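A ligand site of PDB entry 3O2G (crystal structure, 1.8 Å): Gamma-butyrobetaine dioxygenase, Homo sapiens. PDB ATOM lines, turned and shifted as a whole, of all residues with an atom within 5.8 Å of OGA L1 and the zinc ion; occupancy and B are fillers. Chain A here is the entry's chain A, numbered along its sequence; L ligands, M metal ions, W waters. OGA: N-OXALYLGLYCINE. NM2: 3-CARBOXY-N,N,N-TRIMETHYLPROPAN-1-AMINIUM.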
ATOM      1  N   TRP A 182     -22.392 -11.686  14.639  1.00  0.00           N
ATOM      2  CA  TRP A 182     -21.550 -10.891  13.762  1.00  0.00           C
ATOM      3  C   TRP A 182     -21.390 -11.580  12.394  1.00  0.00           C
ATOM      4  O   TRP A 182     -21.502 -12.830  12.285  1.00  0.00           O
ATOM      5  CB  TRP A 182     -20.197 -10.604  14.402  1.00  0.00           C
ATOM      6  CG  TRP A 182     -19.732 -11.666  15.353  1.00  0.00           C
ATOM      7  CD1 TRP A 182     -19.954 -11.675  16.691  1.00  0.00           C
ATOM      8  CD2 TRP A 182     -18.977 -12.864  15.061  1.00  0.00           C
ATOM      9  NE1 TRP A 182     -19.391 -12.806  17.256  1.00  0.00           N
ATOM     10  CE2 TRP A 182     -18.783 -13.544  16.301  1.00  0.00           C
ATOM     11  CE3 TRP A 182     -18.434 -13.421  13.905  1.00  0.00           C
ATOM     12  CZ2 TRP A 182     -18.090 -14.743  16.392  1.00  0.00           C
ATOM     13  CZ3 TRP A 182     -17.741 -14.620  13.997  1.00  0.00           C
ATOM     14  CH2 TRP A 182     -17.575 -15.280  15.243  1.00  0.00           C
ATOM     15  N   VAL A 184     -19.134 -12.383   9.186  1.00  0.00           N
ATOM     16  CA  VAL A 184     -17.791 -12.524   8.683  1.00  0.00           C
ATOM     17  C   VAL A 184     -17.870 -12.401   7.169  1.00  0.00           C
ATOM     18  O   VAL A 184     -18.296 -13.326   6.500  1.00  0.00           O
ATOM     19  CB  VAL A 184     -17.137 -13.848   9.107  1.00  0.00           C
ATOM     20  CG1 VAL A 184     -15.685 -13.891   8.585  1.00  0.00           C
ATOM     21  CG2 VAL A 184     -17.227 -14.034  10.639  1.00  0.00           C
ATOM     22  N   ASN A 192     -11.515  -5.261  11.749  1.00  0.00           N
ATOM     23  CA  ASN A 192     -10.946  -6.513  12.242  1.00  0.00           C
ATOM     24  C   ASN A 192     -10.432  -7.316  11.028  1.00  0.00           C
ATOM     25  O   ASN A 192     -11.055  -7.280   9.977  1.00  0.00           O
ATOM     26  CB  ASN A 192     -12.015  -7.310  13.033  1.00  0.00           C
ATOM     27  CG  ASN A 192     -11.424  -8.477  13.850  1.00  0.00           C
ATOM     28  OD1 ASN A 192     -11.055  -9.499  13.287  1.00  0.00           O
ATOM     29  ND2 ASN A 192     -11.373  -8.335  15.195  1.00  0.00           N
ATOM     30  N   ALA A 194     -10.544 -10.338  10.438  1.00  0.00           N
ATOM     31  CA  ALA A 194     -11.619 -11.278  10.104  1.00  0.00           C
ATOM     32  C   ALA A 194     -12.504 -10.776   8.939  1.00  0.00           C
ATOM     33  O   ALA A 194     -12.967 -11.561   8.101  1.00  0.00           O
ATOM     34  CB  ALA A 194     -12.499 -11.527  11.345  1.00  0.00           C
ATOM     35  N   TYR A 195     -12.747  -9.462   8.893  1.00  0.00           N
ATOM     36  CA  TYR A 195     -13.674  -8.864   7.956  1.00  0.00           C
ATOM     37  C   TYR A 195     -12.946  -8.397   6.690  1.00  0.00           C
ATOM     38  O   TYR A 195     -13.235  -7.346   6.161  1.00  0.00           O
ATOM     39  CB  TYR A 195     -14.426  -7.720   8.605  1.00  0.00           C
ATOM     40  CG  TYR A 195     -15.210  -8.111   9.863  1.00  0.00           C
ATOM     41  CD1 TYR A 195     -15.730  -9.408  10.044  1.00  0.00           C
ATOM     42  CD2 TYR A 195     -15.439  -7.189  10.874  1.00  0.00           C
ATOM     43  CE1 TYR A 195     -16.435  -9.758  11.193  1.00  0.00           C
ATOM     44  CE2 TYR A 195     -16.129  -7.544  12.042  1.00  0.00           C
ATOM     45  CZ  TYR A 195     -16.652  -8.815  12.160  1.00  0.00           C
ATOM     46  OH  TYR A 195     -17.375  -9.218  13.269  1.00  0.00           O
ATOM     47  N   LEU A 200      -6.447 -16.190   7.740  1.00  0.00           N
ATOM     48  CA  LEU A 200      -6.357 -16.165   9.182  1.00  0.00           C
ATOM     49  C   LEU A 200      -5.587 -17.410   9.549  1.00  0.00           C
ATOM     50  O   LEU A 200      -6.023 -18.552   9.211  1.00  0.00           O
ATOM     51  CB  LEU A 200      -7.753 -16.163   9.804  1.00  0.00           C
ATOM     52  CG  LEU A 200      -8.712 -15.030   9.391  1.00  0.00           C
ATOM     53  CD1 LEU A 200     -10.023 -15.133  10.183  1.00  0.00           C
ATOM     54  CD2 LEU A 200      -8.007 -13.650   9.593  1.00  0.00           C
ATOM     55  N   HIS A 203      -5.732 -19.246  15.378  1.00  0.00           N
ATOM     56  CA  HIS A 203      -5.999 -18.330  16.462  1.00  0.00           C
ATOM     57  C   HIS A 203      -7.135 -18.865  17.323  1.00  0.00           C
ATOM     58  O   HIS A 203      -7.895 -19.718  16.894  1.00  0.00           O
ATOM     59  CB  HIS A 203      -6.394 -16.925  15.977  1.00  0.00           C
ATOM     60  CG  HIS A 203      -7.670 -16.868  15.196  1.00  0.00           C
ATOM     61  ND1 HIS A 203      -7.763 -17.320  13.912  1.00  0.00           N
ATOM     62  CD2 HIS A 203      -8.912 -16.436  15.546  1.00  0.00           C
ATOM     63  CE1 HIS A 203      -9.008 -17.151  13.474  1.00  0.00           C
ATOM     64  NE2 HIS A 203      -9.727 -16.615  14.448  1.00  0.00           N
ATOM     65  N   THR A 204      -7.225 -18.336  18.534  1.00  0.00           N
ATOM     66  CA  THR A 204      -8.437 -18.338  19.358  1.00  0.00           C
ATOM     67  C   THR A 204      -9.088 -16.952  19.177  1.00  0.00           C
ATOM     68  O   THR A 204      -8.402 -15.989  18.929  1.00  0.00           O
ATOM     69  CB  THR A 204      -8.116 -18.637  20.869  1.00  0.00           C
ATOM     70  OG1 THR A 204      -7.281 -17.613  21.416  1.00  0.00           O
ATOM     71  CG2 THR A 204      -7.416 -19.986  21.019  1.00  0.00           C
ATOM     72  N   ASP A 205     -10.417 -16.871  19.278  1.00  0.00           N
ATOM     73  CA  ASP A 205     -11.127 -15.633  19.182  1.00  0.00           C
ATOM     74  C   ASP A 205     -11.067 -14.916  20.505  1.00  0.00           C
ATOM     75  O   ASP A 205     -11.279 -15.479  21.579  1.00  0.00           O
ATOM     76  CB  ASP A 205     -12.594 -15.859  18.780  1.00  0.00           C
ATOM     77  CG  ASP A 205     -12.801 -15.813  17.294  1.00  0.00           C
ATOM     78  OD1 ASP A 205     -11.880 -16.198  16.596  1.00  0.00           O
ATOM     79  OD2 ASP A 205     -13.879 -15.328  16.860  1.00  0.00           O
ATOM     80  N   GLN A 216     -17.678 -21.072  20.462  1.00  0.00           N
ATOM     81  CA  GLN A 216     -17.924 -20.305  19.258  1.00  0.00           C
ATOM     82  C   GLN A 216     -18.890 -21.075  18.334  1.00  0.00           C
ATOM     83  O   GLN A 216     -18.784 -22.287  18.177  1.00  0.00           O
ATOM     84  CB  GLN A 216     -16.611 -20.017  18.538  1.00  0.00           C
ATOM     85  CG  GLN A 216     -16.787 -19.135  17.350  1.00  0.00           C
ATOM     86  CD  GLN A 216     -15.503 -18.834  16.614  1.00  0.00           C
ATOM     87  OE1 GLN A 216     -15.549 -18.582  15.430  1.00  0.00           O
ATOM     88  NE2 GLN A 216     -14.350 -18.804  17.335  1.00  0.00           N
ATOM     89  N   LEU A 218     -20.291 -20.858  14.336  1.00  0.00           N
ATOM     90  CA  LEU A 218     -20.018 -20.247  13.022  1.00  0.00           C
ATOM     91  C   LEU A 218     -20.857 -20.948  11.961  1.00  0.00           C
ATOM     92  O   LEU A 218     -20.726 -22.145  11.733  1.00  0.00           O
ATOM     93  CB  LEU A 218     -18.552 -20.330  12.625  1.00  0.00           C
ATOM     94  CG  LEU A 218     -17.493 -19.295  13.010  1.00  0.00           C
ATOM     95  CD1 LEU A 218     -16.126 -19.724  12.391  1.00  0.00           C
ATOM     96  CD2 LEU A 218     -17.808 -17.864  12.642  1.00  0.00           C
ATOM     97  N   GLY A 228     -11.057 -19.882   1.152  1.00  0.00           N
ATOM     98  CA  GLY A 228     -11.905 -19.848   2.312  1.00  0.00           C
ATOM     99  C   GLY A 228     -12.148 -21.154   3.046  1.00  0.00           C
ATOM    100  O   GLY A 228     -13.119 -21.265   3.808  1.00  0.00           O
ATOM    101  N   ASP A 229     -11.295 -22.146   2.795  1.00  0.00           N
ATOM    102  CA  ASP A 229     -11.347 -23.384   3.563  1.00  0.00           C
ATOM    103  C   ASP A 229     -11.029 -23.115   5.028  1.00  0.00           C
ATOM    104  O   ASP A 229     -10.310 -22.153   5.371  1.00  0.00           O
ATOM    105  CB  ASP A 229     -10.359 -24.420   3.013  1.00  0.00           C
ATOM    106  CG  ASP A 229     -10.596 -24.741   1.561  1.00  0.00           C
ATOM    107  OD1 ASP A 229     -10.449 -23.827   0.705  1.00  0.00           O
ATOM    108  OD2 ASP A 229     -10.897 -25.914   1.254  1.00  0.00           O
ATOM    109  N   SER A 230     -11.582 -23.951   5.882  1.00  0.00           N
ATOM    110  CA  SER A 230     -11.419 -23.866   7.331  1.00  0.00           C
ATOM    111  C   SER A 230     -10.308 -24.838   7.752  1.00  0.00           C
ATOM    112  O   SER A 230     -10.072 -25.852   7.108  1.00  0.00           O
ATOM    113  CB  SER A 230     -12.728 -24.257   8.009  1.00  0.00           C
ATOM    114  OG  SER A 230     -13.783 -23.363   7.706  1.00  0.00           O
ATOM    115  N   MET A 333     -16.464 -25.368   4.674  1.00  0.00           N
ATOM    116  CA  MET A 333     -17.883 -25.182   5.013  1.00  0.00           C
ATOM    117  C   MET A 333     -18.718 -24.922   3.778  1.00  0.00           C
ATOM    118  O   MET A 333     -18.274 -24.202   2.869  1.00  0.00           O
ATOM    119  CB  MET A 333     -18.069 -24.017   5.989  1.00  0.00           C
ATOM    120  CG  MET A 333     -17.317 -24.209   7.318  1.00  0.00           C
ATOM    121  SD  MET A 333     -17.804 -23.054   8.601  1.00  0.00           S
ATOM    122  CE  MET A 333     -19.422 -23.662   9.027  1.00  0.00           C
ATOM    123  N   HIS A 348      -8.331 -22.154  15.306  1.00  0.00           N
ATOM    124  CA  HIS A 348      -9.008 -22.239  14.002  1.00  0.00           C
ATOM    125  C   HIS A 348      -8.435 -21.190  13.077  1.00  0.00           C
ATOM    126  O   HIS A 348      -7.762 -20.230  13.512  1.00  0.00           O
ATOM    127  CB  HIS A 348     -10.521 -22.114  14.136  1.00  0.00           C
ATOM    128  CG  HIS A 348     -10.967 -20.817  14.707  1.00  0.00           C
ATOM    129  ND1 HIS A 348     -10.752 -20.468  16.032  1.00  0.00           N
ATOM    130  CD2 HIS A 348     -11.521 -19.725  14.110  1.00  0.00           C
ATOM    131  CE1 HIS A 348     -11.206 -19.235  16.235  1.00  0.00           C
ATOM    132  NE2 HIS A 348     -11.670 -18.762  15.091  1.00  0.00           N
ATOM    133  N   GLY A 349      -8.646 -21.414  11.793  1.00  0.00           N
ATOM    134  CA  GLY A 349      -8.125 -20.505  10.787  1.00  0.00           C
ATOM    135  C   GLY A 349      -8.897 -20.627   9.495  1.00  0.00           C
ATOM    136  O   GLY A 349      -9.794 -21.503   9.345  1.00  0.00           O
ATOM    137  N   ARG A 350      -8.542 -19.769   8.551  1.00  0.00           N
ATOM    138  CA  ARG A 350      -9.157 -19.847   7.251  1.00  0.00           C
ATOM    139  C   ARG A 350      -8.182 -19.417   6.155  1.00  0.00           C
ATOM    140  O   ARG A 350      -7.350 -18.561   6.370  1.00  0.00           O
ATOM    141  CB  ARG A 350     -10.420 -19.025   7.185  1.00  0.00           C
ATOM    142  CG  ARG A 350     -10.260 -17.563   7.292  1.00  0.00           C
ATOM    143  CD  ARG A 350     -11.127 -16.804   6.234  1.00  0.00           C
ATOM    144  NE  ARG A 350     -10.614 -15.457   6.216  1.00  0.00           N
ATOM    145  CZ  ARG A 350     -11.165 -14.361   6.763  1.00  0.00           C
ATOM    146  NH1 ARG A 350     -12.357 -14.348   7.359  1.00  0.00           N
ATOM    147  NH2 ARG A 350     -10.486 -13.224   6.674  1.00  0.00           N
ATOM    148  N   ARG A 361     -18.795 -14.484   0.091  1.00  0.00           N
ATOM    149  CA  ARG A 361     -18.578 -15.309   1.284  1.00  0.00           C
ATOM    150  C   ARG A 361     -19.105 -14.567   2.506  1.00  0.00           C
ATOM    151  O   ARG A 361     -18.830 -13.380   2.676  1.00  0.00           O
ATOM    152  CB  ARG A 361     -17.080 -15.654   1.469  1.00  0.00           C
ATOM    153  CG  ARG A 361     -16.813 -16.755   2.499  1.00  0.00           C
ATOM    154  CD  ARG A 361     -15.315 -16.980   2.624  1.00  0.00           C
ATOM    155  NE  ARG A 361     -14.935 -18.103   3.486  1.00  0.00           N
ATOM    156  CZ  ARG A 361     -14.766 -18.062   4.802  1.00  0.00           C
ATOM    157  NH1 ARG A 361     -15.001 -16.967   5.518  1.00  0.00           N
ATOM    158  NH2 ARG A 361     -14.379 -19.168   5.442  1.00  0.00           N
ATOM    159  N   LEU A 363     -20.188 -15.683   6.666  1.00  0.00           N
ATOM    160  CA  LEU A 363     -20.512 -16.487   7.812  1.00  0.00           C
ATOM    161  C   LEU A 363     -21.201 -15.603   8.877  1.00  0.00           C
ATOM    162  O   LEU A 363     -20.872 -14.408   9.014  1.00  0.00           O
ATOM    163  CB  LEU A 363     -19.257 -17.124   8.399  1.00  0.00           C
ATOM    164  CG  LEU A 363     -18.205 -17.649   7.433  1.00  0.00           C
ATOM    165  CD1 LEU A 363     -17.007 -18.207   8.267  1.00  0.00           C
ATOM    166  CD2 LEU A 363     -18.792 -18.683   6.474  1.00  0.00           C
ATOM    167  N   TYR A 367     -21.005 -16.247  20.129  1.00  0.00           N
ATOM    168  CA  TYR A 367     -20.304 -16.873  21.242  1.00  0.00           C
ATOM    169  C   TYR A 367     -21.265 -17.278  22.349  1.00  0.00           C
ATOM    170  O   TYR A 367     -22.372 -16.737  22.467  1.00  0.00           O
ATOM    171  CB  TYR A 367     -19.282 -15.883  21.831  1.00  0.00           C
ATOM    172  CG  TYR A 367     -18.224 -15.342  20.858  1.00  0.00           C
ATOM    173  CD1 TYR A 367     -17.293 -16.172  20.239  1.00  0.00           C
ATOM    174  CD2 TYR A 367     -18.114 -13.970  20.630  1.00  0.00           C
ATOM    175  CE1 TYR A 367     -16.307 -15.668  19.388  1.00  0.00           C
ATOM    176  CE2 TYR A 367     -17.132 -13.440  19.804  1.00  0.00           C
ATOM    177  CZ  TYR A 367     -16.213 -14.304  19.176  1.00  0.00           C
ATOM    178  OH  TYR A 367     -15.242 -13.806  18.308  1.00  0.00           O
HETATM  179  C1  OGA L   1     -12.870 -15.049  12.572  1.00  0.00           C
HETATM  180  C2  OGA L   1     -12.717 -16.397  11.910  1.00  0.00           C
HETATM  181  C4  OGA L   1     -13.137 -17.939  10.123  1.00  0.00           C
HETATM  182  C5  OGA L   1     -13.577 -17.891   8.648  1.00  0.00           C
HETATM  183  O1  OGA L   1     -13.657 -14.248  12.016  1.00  0.00           O
HETATM  184  O2  OGA L   1     -12.213 -14.840  13.640  1.00  0.00           O
HETATM  185  O2' OGA L   1     -12.000 -17.236  12.466  1.00  0.00           O
HETATM  186  O3  OGA L   1     -13.759 -16.756   8.168  1.00  0.00           O
HETATM  187  N1  OGA L   1     -13.310 -16.616  10.738  1.00  0.00           N
HETATM  188  O4  OGA L   1     -13.751 -18.992   8.092  1.00  0.00           O
HETATM  189  N1  NM2 L   2     -14.715 -11.404  15.405  1.00  0.00           N
HETATM  190  C8  NM2 L   2     -15.949 -11.321  16.245  1.00  0.00           C
HETATM  191  O4  NM2 L   2     -10.751 -10.492  17.151  1.00  0.00           O
HETATM  192  C5  NM2 L   2     -10.563 -11.605  17.717  1.00  0.00           C
HETATM  193  O7  NM2 L   2      -9.745 -11.966  18.567  1.00  0.00           O
HETATM  194  C6  NM2 L   2     -11.226 -12.449  16.639  1.00  0.00           C
HETATM  195  C2  NM2 L   2     -13.605 -11.764  16.314  1.00  0.00           C
HETATM  196  C9  NM2 L   2     -14.348 -10.148  14.713  1.00  0.00           C
HETATM  197  C10 NM2 L   2     -14.913 -12.433  14.368  1.00  0.00           C
HETATM  198  C3  NM2 L   2     -12.251 -12.111  15.772  1.00  0.00           C
HETATM  199 ZN    ZN M   1     -11.815 -16.714  14.517  1.00  0.00          ZN
HETATM  200  O   HOH W   1     -13.919 -16.752  14.511  1.00  0.00           O
HETATM  201  O   HOH W   2      -9.443 -13.407  13.518  1.00  0.00           O
HETATM  202  O   HOH W   3     -13.056 -21.269   9.272  1.00  0.00           O
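NE2 of Gln 216 sits close to NE2 of His 348, at 3.5 Å. The side-chain hydroxyl of Tyr 367 lies within hydrogen-bond range of the side-chain carboxylate of Asp 205. The guanidinium group of Arg 361 is in hydrogen-bond range of the backbone carbonyl oxygen of Gly 228 (2.9 Å). O of Ala 194 is in hydrogen-bond range of NH1 of Arg 350 (2.9 Å). The backbone carbonyl oxygen (O) of Leu 200 lies within hydrogen-bond range of the backbone NH (N) of Arg 350 (2.9 Å). The backbone NH of Ala 194 lies within hydrogen-bond range of the side-chain amide oxygen of Asn 192 (3.0 Å). O of Leu 363 sits at hydrogen-bond distance from N of Val 184, 2.7 Å away.
Water W1 bridges OE1 of Gln 216 and OD2 of Asp 205. Water W3 lies within hydrogen-bond range of an oxygen (O4) of OGA L1 (2.7 Å), the side-chain hydroxyl of Ser 230 (2.7 Å) and the backbone carbonyl oxygen of Gly 349 (3.3 Å).
Merely in contact with OGA L1: Ala 194 (3.0 Å), Leu 363 (3.4 Å), Leu 200 (3.4 Å) and Val 184 (3.5 Å). Hydrophobic or aromatic side chains within 4 Å of OGA L1: Val 184, Ala 194, Leu 200, His 203, His 348 and Leu 363. The nearest printed residue that does not touch OGA L1 is Leu 218 (4.2 Å).
O4 of OGA L1 is in salt-bridge range of NH2 of Arg 361 (2.7 Å). The guanidinium group (NH1) of Arg 350 lies within salt-bridge range of an oxygen (O3) of OGA L1. An oxygen (O4) of NM2 L2 lies within hydrogen-bond range of the side-chain amide nitrogen of Asn 192 (3.0 Å).
Three residues have an atom within 4 Å of the zinc ion: His 203, Asp 205 and His 348. Along chain A the residues within 4 Å of the zinc ion span positions 203 to 348. The nearest printed residue that does not touch the zinc ion is Gln 216 (4.3 Å).
The zinc ion is bound by a ring nitrogen (NE2) of His 203 (2.1 Å), water W1 (2.1 Å), an oxygen (O2) of OGA L1 (2.1 Å), an oxygen (O2') of OGA L1 (2.1 Å), a ring nitrogen (NE2) of His 348 (2.1 Å) and the side-chain carboxylate of Asp 205 (2.1 Å).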
